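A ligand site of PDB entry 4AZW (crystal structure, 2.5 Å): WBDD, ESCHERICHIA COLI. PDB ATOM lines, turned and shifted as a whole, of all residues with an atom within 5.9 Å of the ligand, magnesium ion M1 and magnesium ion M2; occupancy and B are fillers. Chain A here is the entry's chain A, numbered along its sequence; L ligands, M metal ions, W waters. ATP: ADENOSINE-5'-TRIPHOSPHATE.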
ATOM      1  N   GLN A 239     -20.562  27.285   5.538  1.00  0.00           N
ATOM      2  CA  GLN A 239     -21.465  28.444   5.554  1.00  0.00           C
ATOM      3  C   GLN A 239     -20.737  29.725   5.786  1.00  0.00           C
ATOM      4  O   GLN A 239     -19.683  29.783   6.407  1.00  0.00           O
ATOM      5  CB  GLN A 239     -22.624  28.297   6.536  1.00  0.00           C
ATOM      6  CG  GLN A 239     -22.218  27.885   7.910  1.00  0.00           C
ATOM      7  CD  GLN A 239     -23.378  27.271   8.738  1.00  0.00           C
ATOM      8  OE1 GLN A 239     -23.699  27.746   9.834  1.00  0.00           O
ATOM      9  NE2 GLN A 239     -23.983  26.210   8.212  1.00  0.00           N
ATOM     10  N   GLN A 241     -22.321  32.248   7.262  1.00  0.00           N
ATOM     11  CA  GLN A 241     -22.877  32.855   8.470  1.00  0.00           C
ATOM     12  C   GLN A 241     -22.927  31.827   9.605  1.00  0.00           C
ATOM     13  O   GLN A 241     -22.942  30.624   9.349  1.00  0.00           O
ATOM     14  CB  GLN A 241     -24.286  33.407   8.207  1.00  0.00           C
ATOM     15  CG  GLN A 241     -25.201  32.393   7.550  1.00  0.00           C
ATOM     16  CD  GLN A 241     -26.592  32.941   7.278  1.00  0.00           C
ATOM     17  OE1 GLN A 241     -26.796  34.154   7.084  1.00  0.00           O
ATOM     18  NE2 GLN A 241     -27.561  32.039   7.251  1.00  0.00           N
ATOM     19  N   PRO A 242     -22.930  32.300  10.853  1.00  0.00           N
ATOM     20  CA  PRO A 242     -22.769  31.350  11.947  1.00  0.00           C
ATOM     21  C   PRO A 242     -23.989  30.445  12.201  1.00  0.00           C
ATOM     22  O   PRO A 242     -23.830  29.307  12.677  1.00  0.00           O
ATOM     23  CB  PRO A 242     -22.390  32.231  13.131  1.00  0.00           C
ATOM     24  CG  PRO A 242     -22.849  33.586  12.782  1.00  0.00           C
ATOM     25  CD  PRO A 242     -22.737  33.681  11.289  1.00  0.00           C
ATOM     26  N   TYR A 243     -25.179  30.921  11.866  1.00  0.00           N
ATOM     27  CA  TYR A 243     -26.420  30.192  12.211  1.00  0.00           C
ATOM     28  C   TYR A 243     -27.594  30.741  11.393  1.00  0.00           C
ATOM     29  O   TYR A 243     -27.560  31.891  10.964  1.00  0.00           O
ATOM     30  CB  TYR A 243     -26.724  30.260  13.746  1.00  0.00           C
ATOM     31  CG  TYR A 243     -26.730  31.664  14.300  1.00  0.00           C
ATOM     32  CD1 TYR A 243     -27.883  32.404  14.308  1.00  0.00           C
ATOM     33  CD2 TYR A 243     -25.605  32.212  14.848  1.00  0.00           C
ATOM     34  CE1 TYR A 243     -27.891  33.695  14.787  1.00  0.00           C
ATOM     35  CE2 TYR A 243     -25.600  33.507  15.330  1.00  0.00           C
ATOM     36  CZ  TYR A 243     -26.741  34.245  15.293  1.00  0.00           C
ATOM     37  OH  TYR A 243     -26.731  35.533  15.763  1.00  0.00           O
ATOM     38  N   ALA A 249     -24.092  40.247  10.012  1.00  0.00           N
ATOM     39  CA  ALA A 249     -23.319  40.912  11.104  1.00  0.00           C
ATOM     40  C   ALA A 249     -21.810  41.008  10.897  1.00  0.00           C
ATOM     41  O   ALA A 249     -21.196  41.976  11.317  1.00  0.00           O
ATOM     42  CB  ALA A 249     -23.599  40.223  12.434  1.00  0.00           C
ATOM     43  N   HIS A 250     -21.220  39.992  10.264  1.00  0.00           N
ATOM     44  CA  HIS A 250     -19.779  39.944  10.053  1.00  0.00           C
ATOM     45  C   HIS A 250     -19.427  40.303   8.641  1.00  0.00           C
ATOM     46  O   HIS A 250     -18.306  40.106   8.172  1.00  0.00           O
ATOM     47  CB  HIS A 250     -19.265  38.574  10.431  1.00  0.00           C
ATOM     48  CG  HIS A 250     -19.594  38.187  11.833  1.00  0.00           C
ATOM     49  ND1 HIS A 250     -19.168  38.901  12.879  1.00  0.00           N
ATOM     50  CD2 HIS A 250     -20.399  37.166  12.354  1.00  0.00           C
ATOM     51  CE1 HIS A 250     -19.650  38.360  14.020  1.00  0.00           C
ATOM     52  NE2 HIS A 250     -20.393  37.297  13.707  1.00  0.00           N
ATOM     53  N   ARG A 254     -16.395  35.948   7.903  1.00  0.00           N
ATOM     54  CA  ARG A 254     -16.079  34.655   8.496  1.00  0.00           C
ATOM     55  C   ARG A 254     -16.696  33.480   7.730  1.00  0.00           C
ATOM     56  O   ARG A 254     -17.856  33.553   7.330  1.00  0.00           O
ATOM     57  CB  ARG A 254     -16.520  34.579   9.949  1.00  0.00           C
ATOM     58  CG  ARG A 254     -16.597  35.936  10.612  1.00  0.00           C
ATOM     59  CD  ARG A 254     -16.506  35.811  12.093  1.00  0.00           C
ATOM     60  NE  ARG A 254     -16.092  37.032  12.716  1.00  0.00           N
ATOM     61  CZ  ARG A 254     -16.160  37.237  14.043  1.00  0.00           C
ATOM     62  NH1 ARG A 254     -16.630  36.286  14.845  1.00  0.00           N
ATOM     63  NH2 ARG A 254     -15.751  38.379  14.546  1.00  0.00           N
ATOM     64  N   TYR A 256     -17.218  29.210   7.884  1.00  0.00           N
ATOM     65  CA  TYR A 256     -17.281  28.047   8.741  1.00  0.00           C
ATOM     66  C   TYR A 256     -17.385  26.752   7.901  1.00  0.00           C
ATOM     67  O   TYR A 256     -18.295  26.627   7.065  1.00  0.00           O
ATOM     68  CB  TYR A 256     -18.502  28.224   9.632  1.00  0.00           C
ATOM     69  CG  TYR A 256     -18.537  29.574  10.339  1.00  0.00           C
ATOM     70  CD1 TYR A 256     -17.758  29.829  11.437  1.00  0.00           C
ATOM     71  CD2 TYR A 256     -19.333  30.602   9.849  1.00  0.00           C
ATOM     72  CE1 TYR A 256     -17.806  31.087  12.063  1.00  0.00           C
ATOM     73  CE2 TYR A 256     -19.394  31.818  10.442  1.00  0.00           C
ATOM     74  CZ  TYR A 256     -18.642  32.088  11.547  1.00  0.00           C
ATOM     75  OH  TYR A 256     -18.741  33.341  12.088  1.00  0.00           O
ATOM     76  N   PHE A 258     -17.466  22.470   7.995  1.00  0.00           N
ATOM     77  CA  PHE A 258     -17.883  21.332   8.826  1.00  0.00           C
ATOM     78  C   PHE A 258     -17.414  20.038   8.180  1.00  0.00           C
ATOM     79  O   PHE A 258     -17.865  19.646   7.076  1.00  0.00           O
ATOM     80  CB  PHE A 258     -19.408  21.263   8.960  1.00  0.00           C
ATOM     81  CG  PHE A 258     -19.987  22.435   9.664  1.00  0.00           C
ATOM     82  CD1 PHE A 258     -20.149  23.624   9.016  1.00  0.00           C
ATOM     83  CD2 PHE A 258     -20.297  22.361  10.987  1.00  0.00           C
ATOM     84  CE1 PHE A 258     -20.620  24.728   9.671  1.00  0.00           C
ATOM     85  CE2 PHE A 258     -20.759  23.446  11.648  1.00  0.00           C
ATOM     86  CZ  PHE A 258     -20.934  24.641  10.991  1.00  0.00           C
ATOM     87  N   VAL A 263     -14.745  21.332  13.178  1.00  0.00           N
ATOM     88  CA  VAL A 263     -15.249  22.578  12.660  1.00  0.00           C
ATOM     89  C   VAL A 263     -14.069  23.539  12.488  1.00  0.00           C
ATOM     90  O   VAL A 263     -13.229  23.664  13.390  1.00  0.00           O
ATOM     91  CB  VAL A 263     -16.301  23.189  13.572  1.00  0.00           C
ATOM     92  CG1 VAL A 263     -16.942  24.396  12.897  1.00  0.00           C
ATOM     93  CG2 VAL A 263     -17.349  22.145  13.872  1.00  0.00           C
ATOM     94  N   LYS A 265     -13.100  27.491  11.750  1.00  0.00           N
ATOM     95  CA  LYS A 265     -13.454  28.902  11.696  1.00  0.00           C
ATOM     96  C   LYS A 265     -12.335  29.595  10.911  1.00  0.00           C
ATOM     97  O   LYS A 265     -11.156  29.431  11.250  1.00  0.00           O
ATOM     98  CB  LYS A 265     -13.559  29.468  13.118  1.00  0.00           C
ATOM     99  CG  LYS A 265     -14.874  29.076  13.803  1.00  0.00           C
ATOM    100  CD  LYS A 265     -14.846  29.239  15.333  1.00  0.00           C
ATOM    101  CE  LYS A 265     -15.631  30.467  15.787  1.00  0.00           C
ATOM    102  NZ  LYS A 265     -15.449  30.751  17.233  1.00  0.00           N
ATOM    103  N   PHE A 267     -11.482  33.307   9.431  1.00  0.00           N
ATOM    104  CA  PHE A 267     -11.819  34.733   9.503  1.00  0.00           C
ATOM    105  C   PHE A 267     -10.892  35.561   8.607  1.00  0.00           C
ATOM    106  O   PHE A 267      -9.682  35.473   8.713  1.00  0.00           O
ATOM    107  CB  PHE A 267     -11.608  35.249  10.951  1.00  0.00           C
ATOM    108  CG  PHE A 267     -12.606  34.735  11.963  1.00  0.00           C
ATOM    109  CD1 PHE A 267     -13.446  33.684  11.700  1.00  0.00           C
ATOM    110  CD2 PHE A 267     -12.672  35.324  13.217  1.00  0.00           C
ATOM    111  CE1 PHE A 267     -14.339  33.231  12.667  1.00  0.00           C
ATOM    112  CE2 PHE A 267     -13.537  34.859  14.201  1.00  0.00           C
ATOM    113  CZ  PHE A 267     -14.392  33.820  13.901  1.00  0.00           C
ATOM    114  N   GLU A 287     -11.436  38.362  18.682  1.00  0.00           N
ATOM    115  CA  GLU A 287     -12.287  37.244  18.935  1.00  0.00           C
ATOM    116  C   GLU A 287     -11.579  35.920  18.623  1.00  0.00           C
ATOM    117  O   GLU A 287     -11.592  35.025  19.461  1.00  0.00           O
ATOM    118  CB  GLU A 287     -13.597  37.396  18.198  1.00  0.00           C
ATOM    119  CG  GLU A 287     -14.546  36.224  18.384  1.00  0.00           C
ATOM    120  CD  GLU A 287     -15.988  36.600  18.180  1.00  0.00           C
ATOM    121  OE1 GLU A 287     -16.229  37.684  17.576  1.00  0.00           O
ATOM    122  OE2 GLU A 287     -16.880  35.840  18.662  1.00  0.00           O
ATOM    123  N   GLU A 291     -10.225  33.093  21.520  1.00  0.00           N
ATOM    124  CA  GLU A 291     -10.730  31.722  21.496  1.00  0.00           C
ATOM    125  C   GLU A 291      -9.620  30.720  21.538  1.00  0.00           C
ATOM    126  O   GLU A 291      -9.674  29.806  22.346  1.00  0.00           O
ATOM    127  CB  GLU A 291     -11.640  31.427  20.279  1.00  0.00           C
ATOM    128  CG  GLU A 291     -12.324  30.051  20.404  1.00  0.00           C
ATOM    129  CD  GLU A 291     -13.475  29.808  19.442  1.00  0.00           C
ATOM    130  OE1 GLU A 291     -13.340  30.295  18.277  1.00  0.00           O
ATOM    131  OE2 GLU A 291     -14.496  29.119  19.880  1.00  0.00           O
ATOM    132  N   PRO A 305     -14.002  21.820  23.745  1.00  0.00           N
ATOM    133  CA  PRO A 305     -13.582  21.121  22.529  1.00  0.00           C
ATOM    134  C   PRO A 305     -12.119  21.325  22.273  1.00  0.00           C
ATOM    135  O   PRO A 305     -11.656  22.453  22.439  1.00  0.00           O
ATOM    136  CB  PRO A 305     -14.380  21.831  21.432  1.00  0.00           C
ATOM    137  CG  PRO A 305     -14.697  23.175  21.970  1.00  0.00           C
ATOM    138  CD  PRO A 305     -14.917  22.945  23.437  1.00  0.00           C
ATOM    139  N   MET A 321     -11.303  23.022  15.384  1.00  0.00           N
ATOM    140  CA  MET A 321     -11.580  22.401  16.712  1.00  0.00           C
ATOM    141  C   MET A 321     -12.479  21.184  16.569  1.00  0.00           C
ATOM    142  O   MET A 321     -13.047  20.945  15.482  1.00  0.00           O
ATOM    143  CB  MET A 321     -12.191  23.396  17.696  1.00  0.00           C
ATOM    144  CG  MET A 321     -13.635  23.763  17.394  1.00  0.00           C
ATOM    145  SD  MET A 321     -14.260  25.212  18.287  1.00  0.00           S
ATOM    146  CE  MET A 321     -14.010  26.568  17.166  1.00  0.00           C
ATOM    147  N   GLU A 322     -12.615  20.416  17.665  1.00  0.00           N
ATOM    148  CA  GLU A 322     -13.429  19.205  17.626  1.00  0.00           C
ATOM    149  C   GLU A 322     -14.923  19.599  17.520  1.00  0.00           C
ATOM    150  O   GLU A 322     -15.355  20.556  18.134  1.00  0.00           O
ATOM    151  CB  GLU A 322     -13.123  18.267  18.810  1.00  0.00           C
ATOM    152  CG  GLU A 322     -13.891  18.588  20.079  1.00  0.00           C
ATOM    153  CD  GLU A 322     -13.677  17.574  21.218  1.00  0.00           C
ATOM    154  OE1 GLU A 322     -12.489  17.196  21.482  1.00  0.00           O
ATOM    155  OE2 GLU A 322     -14.693  17.157  21.832  1.00  0.00           O
ATOM    156  N   LYS A 323     -15.668  18.866  16.713  1.00  0.00           N
ATOM    157  CA  LYS A 323     -17.080  19.125  16.481  1.00  0.00           C
ATOM    158  C   LYS A 323     -17.908  18.467  17.609  1.00  0.00           C
ATOM    159  O   LYS A 323     -17.857  17.262  17.811  1.00  0.00           O
ATOM    160  CB  LYS A 323     -17.466  18.553  15.092  1.00  0.00           C
ATOM    161  CG  LYS A 323     -18.963  18.468  14.788  1.00  0.00           C
ATOM    162  CD  LYS A 323     -19.185  18.391  13.284  1.00  0.00           C
ATOM    163  CE  LYS A 323     -19.916  17.131  12.845  1.00  0.00           C
ATOM    164  NZ  LYS A 323     -20.141  17.156  11.359  1.00  0.00           N
ATOM    165  N   LEU A 324     -18.650  19.291  18.342  1.00  0.00           N
ATOM    166  CA  LEU A 324     -19.504  18.822  19.399  1.00  0.00           C
ATOM    167  C   LEU A 324     -20.757  18.276  18.743  1.00  0.00           C
ATOM    168  O   LEU A 324     -21.111  18.699  17.670  1.00  0.00           O
ATOM    169  CB  LEU A 324     -19.843  19.951  20.352  1.00  0.00           C
ATOM    170  CG  LEU A 324     -18.636  20.576  21.068  1.00  0.00           C
ATOM    171  CD1 LEU A 324     -19.121  21.780  21.841  1.00  0.00           C
ATOM    172  CD2 LEU A 324     -17.865  19.572  21.951  1.00  0.00           C
ATOM    173  N   PRO A 325     -21.382  17.250  19.342  1.00  0.00           N
ATOM    174  CA  PRO A 325     -22.493  16.672  18.620  1.00  0.00           C
ATOM    175  C   PRO A 325     -23.805  17.332  19.070  1.00  0.00           C
ATOM    176  O   PRO A 325     -23.852  17.897  20.159  1.00  0.00           O
ATOM    177  CB  PRO A 325     -22.431  15.189  19.019  1.00  0.00           C
ATOM    178  CG  PRO A 325     -21.883  15.216  20.427  1.00  0.00           C
ATOM    179  CD  PRO A 325     -20.937  16.401  20.469  1.00  0.00           C
ATOM    180  N   LEU A 328     -27.777  23.378  17.549  1.00  0.00           N
ATOM    181  CA  LEU A 328     -27.922  24.620  18.216  1.00  0.00           C
ATOM    182  C   LEU A 328     -29.300  24.725  18.851  1.00  0.00           C
ATOM    183  O   LEU A 328     -30.336  24.420  18.236  1.00  0.00           O
ATOM    184  CB  LEU A 328     -27.719  25.787  17.273  1.00  0.00           C
ATOM    185  CG  LEU A 328     -26.327  25.982  16.700  1.00  0.00           C
ATOM    186  CD1 LEU A 328     -26.357  27.266  15.904  1.00  0.00           C
ATOM    187  CD2 LEU A 328     -25.245  25.982  17.768  1.00  0.00           C
ATOM    188  N   ASP A 364     -21.795  36.005  25.790  1.00  0.00           N
ATOM    189  CA  ASP A 364     -22.726  35.909  24.702  1.00  0.00           C
ATOM    190  C   ASP A 364     -23.496  34.560  24.823  1.00  0.00           C
ATOM    191  O   ASP A 364     -23.521  33.763  23.901  1.00  0.00           O
ATOM    192  CB  ASP A 364     -21.916  36.048  23.410  1.00  0.00           C
ATOM    193  CG  ASP A 364     -22.766  36.343  22.173  1.00  0.00           C
ATOM    194  OD1 ASP A 364     -23.918  36.843  22.245  1.00  0.00           O
ATOM    195  OD2 ASP A 364     -22.221  36.028  21.098  1.00  0.00           O
ATOM    196  N   TRP A 368     -28.167  30.484  20.102  1.00  0.00           N
ATOM    197  CA  TRP A 368     -27.328  30.160  18.963  1.00  0.00           C
ATOM    198  C   TRP A 368     -25.895  29.889  19.293  1.00  0.00           C
ATOM    199  O   TRP A 368     -25.148  29.547  18.376  1.00  0.00           O
ATOM    200  CB  TRP A 368     -27.426  31.240  17.872  1.00  0.00           C
ATOM    201  CG  TRP A 368     -27.299  32.644  18.373  1.00  0.00           C
ATOM    202  CD1 TRP A 368     -26.137  33.378  18.555  1.00  0.00           C
ATOM    203  CD2 TRP A 368     -28.391  33.545  18.824  1.00  0.00           C
ATOM    204  NE1 TRP A 368     -26.424  34.615  19.061  1.00  0.00           N
ATOM    205  CE2 TRP A 368     -27.745  34.778  19.263  1.00  0.00           C
ATOM    206  CE3 TRP A 368     -29.776  33.428  18.943  1.00  0.00           C
ATOM    207  CZ2 TRP A 368     -28.467  35.864  19.725  1.00  0.00           C
ATOM    208  CZ3 TRP A 368     -30.493  34.521  19.437  1.00  0.00           C
ATOM    209  CH2 TRP A 368     -29.852  35.708  19.815  1.00  0.00           C
ATOM    210  N   ASN A 369     -25.507  30.039  20.566  1.00  0.00           N
ATOM    211  CA  ASN A 369     -24.206  29.578  21.061  1.00  0.00           C
ATOM    212  C   ASN A 369     -24.301  28.454  22.070  1.00  0.00           C
ATOM    213  O   ASN A 369     -23.376  28.261  22.890  1.00  0.00           O
ATOM    214  CB  ASN A 369     -23.425  30.738  21.725  1.00  0.00           C
ATOM    215  CG  ASN A 369     -23.087  31.825  20.749  1.00  0.00           C
ATOM    216  OD1 ASN A 369     -22.913  31.543  19.561  1.00  0.00           O
ATOM    217  ND2 ASN A 369     -23.045  33.094  21.224  1.00  0.00           N
ATOM    218  N   MET A 371     -24.957  24.329  22.230  1.00  0.00           N
ATOM    219  CA  MET A 371     -25.162  23.062  21.550  1.00  0.00           C
ATOM    220  C   MET A 371     -25.786  22.053  22.505  1.00  0.00           C
ATOM    221  O   MET A 371     -25.274  21.888  23.656  1.00  0.00           O
ATOM    222  CB  MET A 371     -23.877  22.476  21.007  1.00  0.00           C
ATOM    223  CG  MET A 371     -24.129  21.466  19.889  1.00  0.00           C
ATOM    224  SD  MET A 371     -24.007  22.229  18.257  1.00  0.00           S
ATOM    225  CE  MET A 371     -23.259  23.743  18.859  1.00  0.00           C
ATOM    226  N   ILE A 381     -20.535  26.919  23.114  1.00  0.00           N
ATOM    227  CA  ILE A 381     -19.534  26.998  22.044  1.00  0.00           C
ATOM    228  C   ILE A 381     -19.211  28.502  21.953  1.00  0.00           C
ATOM    229  O   ILE A 381     -19.556  29.257  22.896  1.00  0.00           O
ATOM    230  CB  ILE A 381     -20.055  26.369  20.729  1.00  0.00           C
ATOM    231  CG1 ILE A 381     -21.235  27.166  20.147  1.00  0.00           C
ATOM    232  CG2 ILE A 381     -20.447  24.929  20.980  1.00  0.00           C
ATOM    233  CD1 ILE A 381     -21.638  26.702  18.768  1.00  0.00           C
ATOM    234  N   ASP A 382     -18.540  28.932  20.883  1.00  0.00           N
ATOM    235  CA  ASP A 382     -18.213  30.366  20.688  1.00  0.00           C
ATOM    236  C   ASP A 382     -17.397  30.917  21.900  1.00  0.00           C
ATOM    237  O   ASP A 382     -17.770  31.911  22.575  1.00  0.00           O
ATOM    238  CB  ASP A 382     -19.493  31.162  20.399  1.00  0.00           C
ATOM    239  CG  ASP A 382     -19.245  32.490  19.674  1.00  0.00           C
ATOM    240  OD1 ASP A 382     -18.212  33.165  19.966  1.00  0.00           O
ATOM    241  OD2 ASP A 382     -20.124  32.909  18.824  1.00  0.00           O
ATOM    242  N   PHE A 383     -16.267  30.280  22.157  1.00  0.00           N
ATOM    243  CA  PHE A 383     -15.406  30.660  23.327  1.00  0.00           C
ATOM    244  C   PHE A 383     -14.517  31.873  23.138  1.00  0.00           C
ATOM    245  O   PHE A 383     -13.820  32.277  24.039  1.00  0.00           O
ATOM    246  CB  PHE A 383     -14.556  29.487  23.780  1.00  0.00           C
ATOM    247  CG  PHE A 383     -15.335  28.390  24.370  1.00  0.00           C
ATOM    248  CD1 PHE A 383     -15.906  28.534  25.613  1.00  0.00           C
ATOM    249  CD2 PHE A 383     -15.544  27.230  23.655  1.00  0.00           C
ATOM    250  CE1 PHE A 383     -16.653  27.519  26.161  1.00  0.00           C
ATOM    251  CE2 PHE A 383     -16.278  26.198  24.192  1.00  0.00           C
ATOM    252  CZ  PHE A 383     -16.826  26.352  25.430  1.00  0.00           C
ATOM    253  N   GLY A 384     -14.561  32.477  21.971  1.00  0.00           N
ATOM    254  CA  GLY A 384     -14.059  33.815  21.834  1.00  0.00           C
ATOM    255  C   GLY A 384     -14.959  34.810  22.558  1.00  0.00           C
ATOM    256  O   GLY A 384     -14.608  36.004  22.647  1.00  0.00           O
ATOM    257  N   SER A 385     -16.116  34.358  23.080  1.00  0.00           N
ATOM    258  CA  SER A 385     -16.949  35.214  23.940  1.00  0.00           C
ATOM    259  C   SER A 385     -16.487  35.217  25.413  1.00  0.00           C
ATOM    260  O   SER A 385     -17.099  35.871  26.261  1.00  0.00           O
ATOM    261  CB  SER A 385     -18.405  34.784  23.856  1.00  0.00           C
ATOM    262  OG  SER A 385     -18.845  34.752  22.492  1.00  0.00           O
HETATM  263  PG  ATP L   1     -21.109  34.704  16.346  1.00  0.00           P
HETATM  264  O1G ATP L   1     -21.601  35.750  15.391  1.00  0.00           O
HETATM  265  O2G ATP L   1     -22.168  33.711  16.818  1.00  0.00           O
HETATM  266  O3G ATP L   1     -20.301  35.399  17.426  1.00  0.00           O
HETATM  267  PB  ATP L   1     -18.636  33.203  15.708  1.00  0.00           P
HETATM  268  O1B ATP L   1     -18.217  33.495  17.126  1.00  0.00           O
HETATM  269  O2B ATP L   1     -17.750  33.571  14.548  1.00  0.00           O
HETATM  270  O3B ATP L   1     -20.107  33.829  15.398  1.00  0.00           O
HETATM  271  PA  ATP L   1     -19.293  30.500  16.473  1.00  0.00           P
HETATM  272  O1A ATP L   1     -20.673  30.911  16.916  1.00  0.00           O
HETATM  273  O2A ATP L   1     -18.304  30.008  17.471  1.00  0.00           O
HETATM  274  O3A ATP L   1     -18.645  31.595  15.506  1.00  0.00           O
HETATM  275  O5' ATP L   1     -19.401  29.275  15.450  1.00  0.00           O
HETATM  276  C5' ATP L   1     -20.175  29.367  14.275  1.00  0.00           C
HETATM  277  C4' ATP L   1     -21.074  28.157  14.103  1.00  0.00           C
HETATM  278  O4' ATP L   1     -20.322  26.928  13.916  1.00  0.00           O
HETATM  279  C3' ATP L   1     -21.941  27.934  15.334  1.00  0.00           C
HETATM  280  O3' ATP L   1     -23.135  28.686  15.347  1.00  0.00           O
HETATM  281  C2' ATP L   1     -22.185  26.459  15.245  1.00  0.00           C
HETATM  282  O2' ATP L   1     -23.165  26.186  14.277  1.00  0.00           O
HETATM  283  C1' ATP L   1     -20.899  25.883  14.721  1.00  0.00           C
HETATM  284  N9  ATP L   1     -19.868  25.476  15.722  1.00  0.00           N
HETATM  285  C8  ATP L   1     -18.830  26.222  16.140  1.00  0.00           C
HETATM  286  N7  ATP L   1     -18.004  25.508  16.961  1.00  0.00           N
HETATM  287  C5  ATP L   1     -18.524  24.261  17.017  1.00  0.00           C
HETATM  288  C6  ATP L   1     -18.177  23.011  17.683  1.00  0.00           C
HETATM  289  N6  ATP L   1     -17.102  22.967  18.469  1.00  0.00           N
HETATM  290  N1  ATP L   1     -18.973  21.948  17.519  1.00  0.00           N
HETATM  291  C2  ATP L   1     -20.071  21.972  16.719  1.00  0.00           C
HETATM  292  N3  ATP L   1     -20.444  23.079  16.088  1.00  0.00           N
HETATM  293  C4  ATP L   1     -19.750  24.239  16.229  1.00  0.00           C
HETATM  294 MG    MG M   1     -21.883  31.899  17.920  1.00  0.00          MG
HETATM  295 MG    MG M   2     -18.844  34.873  18.649  1.00  0.00          MG
HETATM  296  O   HOH W   1     -24.923  26.819  12.190  1.00  0.00           O
HETATM  297  O   HOH W   2     -23.913  23.134  14.064  1.00  0.00           O
HETATM  298  O   HOH W   3     -19.848  35.578  20.417  1.00  0.00           O
HETATM  299  O   HOH W   4     -23.304  30.797  16.987  1.00  0.00           O
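Magnesium ion M1 is bound by O1A of the ligand (1.9 Å), OD1 of Asn 369 (2.0 Å), water W4 (2.0 Å), O2G of the ligand (2.1 Å) and OD2 of Asp 382 (2.2 Å).
Magnesium ion M1 has five donor atoms within binding distance.
An oxygen (O3G) of the ligand is bound to magnesium ion M2 (2.0 Å).
Magnesium ion M2 is bound by O1B of the ligand (2.1 Å).
Magnesium ion M2 is bound by water W3, 2.2 Å away.
OE2 of Glu 287 binds magnesium ion M2 (2.2 Å).
Magnesium ion M2 is bound by OD1 of Asp 382, 2.2 Å away.
OD2 of Asp 382 is bound to magnesium ion M2 (2.4 Å).
Magnesium ion M2 has six donor atoms within binding distance.
Water W4 lies within hydrogen-bond range of the backbone carbonyl oxygen of Trp 368 (2.6 Å) and an oxygen (O3') of the ligand (2.7 Å).
Water W3 bridges the side-chain hydroxyl (OG) of Ser 385 (2.4 Å) and the side-chain carboxylate (OD2) of Asp 364 (2.5 Å).
Water W1 lies within hydrogen-bond range of the backbone carbonyl oxygen (O) of Pro 242, an oxygen (O2') of the ligand and the side-chain amide oxygen (OE1) of Gln 239.
NE2 of His 250 lies within hydrogen-bond range of O1G of the ligand, 2.6 Å away.
An oxygen (O2B) of the ligand is in hydrogen-bond range of the side-chain hydroxyl of Tyr 256 (2.7 Å).
N of Leu 324 is in hydrogen-bond range of N1 of the ligand, at 2.8 Å.
The backbone carbonyl oxygen (O) of Pro 242 lies within hydrogen-bond range of an oxygen (O3') of the ligand, 2.8 Å away.
The guanidinium group of Arg 254 lies within salt-bridge range of an oxygen (O2B) of the ligand (3.0 Å).
O2A of the ligand is in salt-bridge range of NZ of Lys 265 (3.0 Å).
The backbone carbonyl oxygen of Glu 322 is in hydrogen-bond range of a nitrogen (N6) of the ligand.
SD of Met 321 lies within hydrogen-bond range of N6 of the ligand, at 3.6 Å.
Merely in contact with the ligand: Tyr 243 (3.7 Å), Phe 258 (3.8 Å), Val 263 (3.9 Å), Phe 267 (3.4 Å), Lys 323 (3.6 Å), Leu 328 (3.6 Å), Trp 368 (3.7 Å) and Ile 381 (3.6 Å).
Hydrophobic or aromatic side chains that line the ligand: Pro 242, Tyr 243, His 250, Tyr 256, Phe 258, Val 263, Phe 267, Met 321, Leu 324, Leu 328 and Ile 381.
Two residues have an atom within 4 Å of magnesium ion M1: Asn 369 and Asp 382.
Residues that only touch magnesium ion M2: Ser 385 (3.8 Å).
Three residues have an atom within 4 Å of magnesium ion M2: Glu 287, Asp 382 and Ser 385.
The backbone carbonyl oxygen (O) of Asn 369 is in hydrogen-bond range of the backbone NH (N) of Ile 381 (3.1 Å).
O of Asp 364 is in hydrogen-bond range of ND2 of Asn 369 (2.8 Å).
The side-chain hydroxyl of Ser 385 is in hydrogen-bond range of the backbone carbonyl oxygen of Asp 382.
The backbone carbonyl oxygen (O) of Tyr 256 lies within hydrogen-bond range of the backbone NH (N) of Gln 239, at 2.8 Å.
OE1 of Gln 239 sits close to O of Pro 242, 3.2 Å away.
The side-chain carboxylate of Glu 291 lies within salt-bridge range of the side-chain amino group of Lys 265 (3.3 Å).
N of Met 321 is in hydrogen-bond range of O of Val 263 (2.8 Å).
The indole nitrogen (NE1) of Trp 368 is in hydrogen-bond range of the side-chain hydroxyl (OH) of Tyr 243 (3.4 Å).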
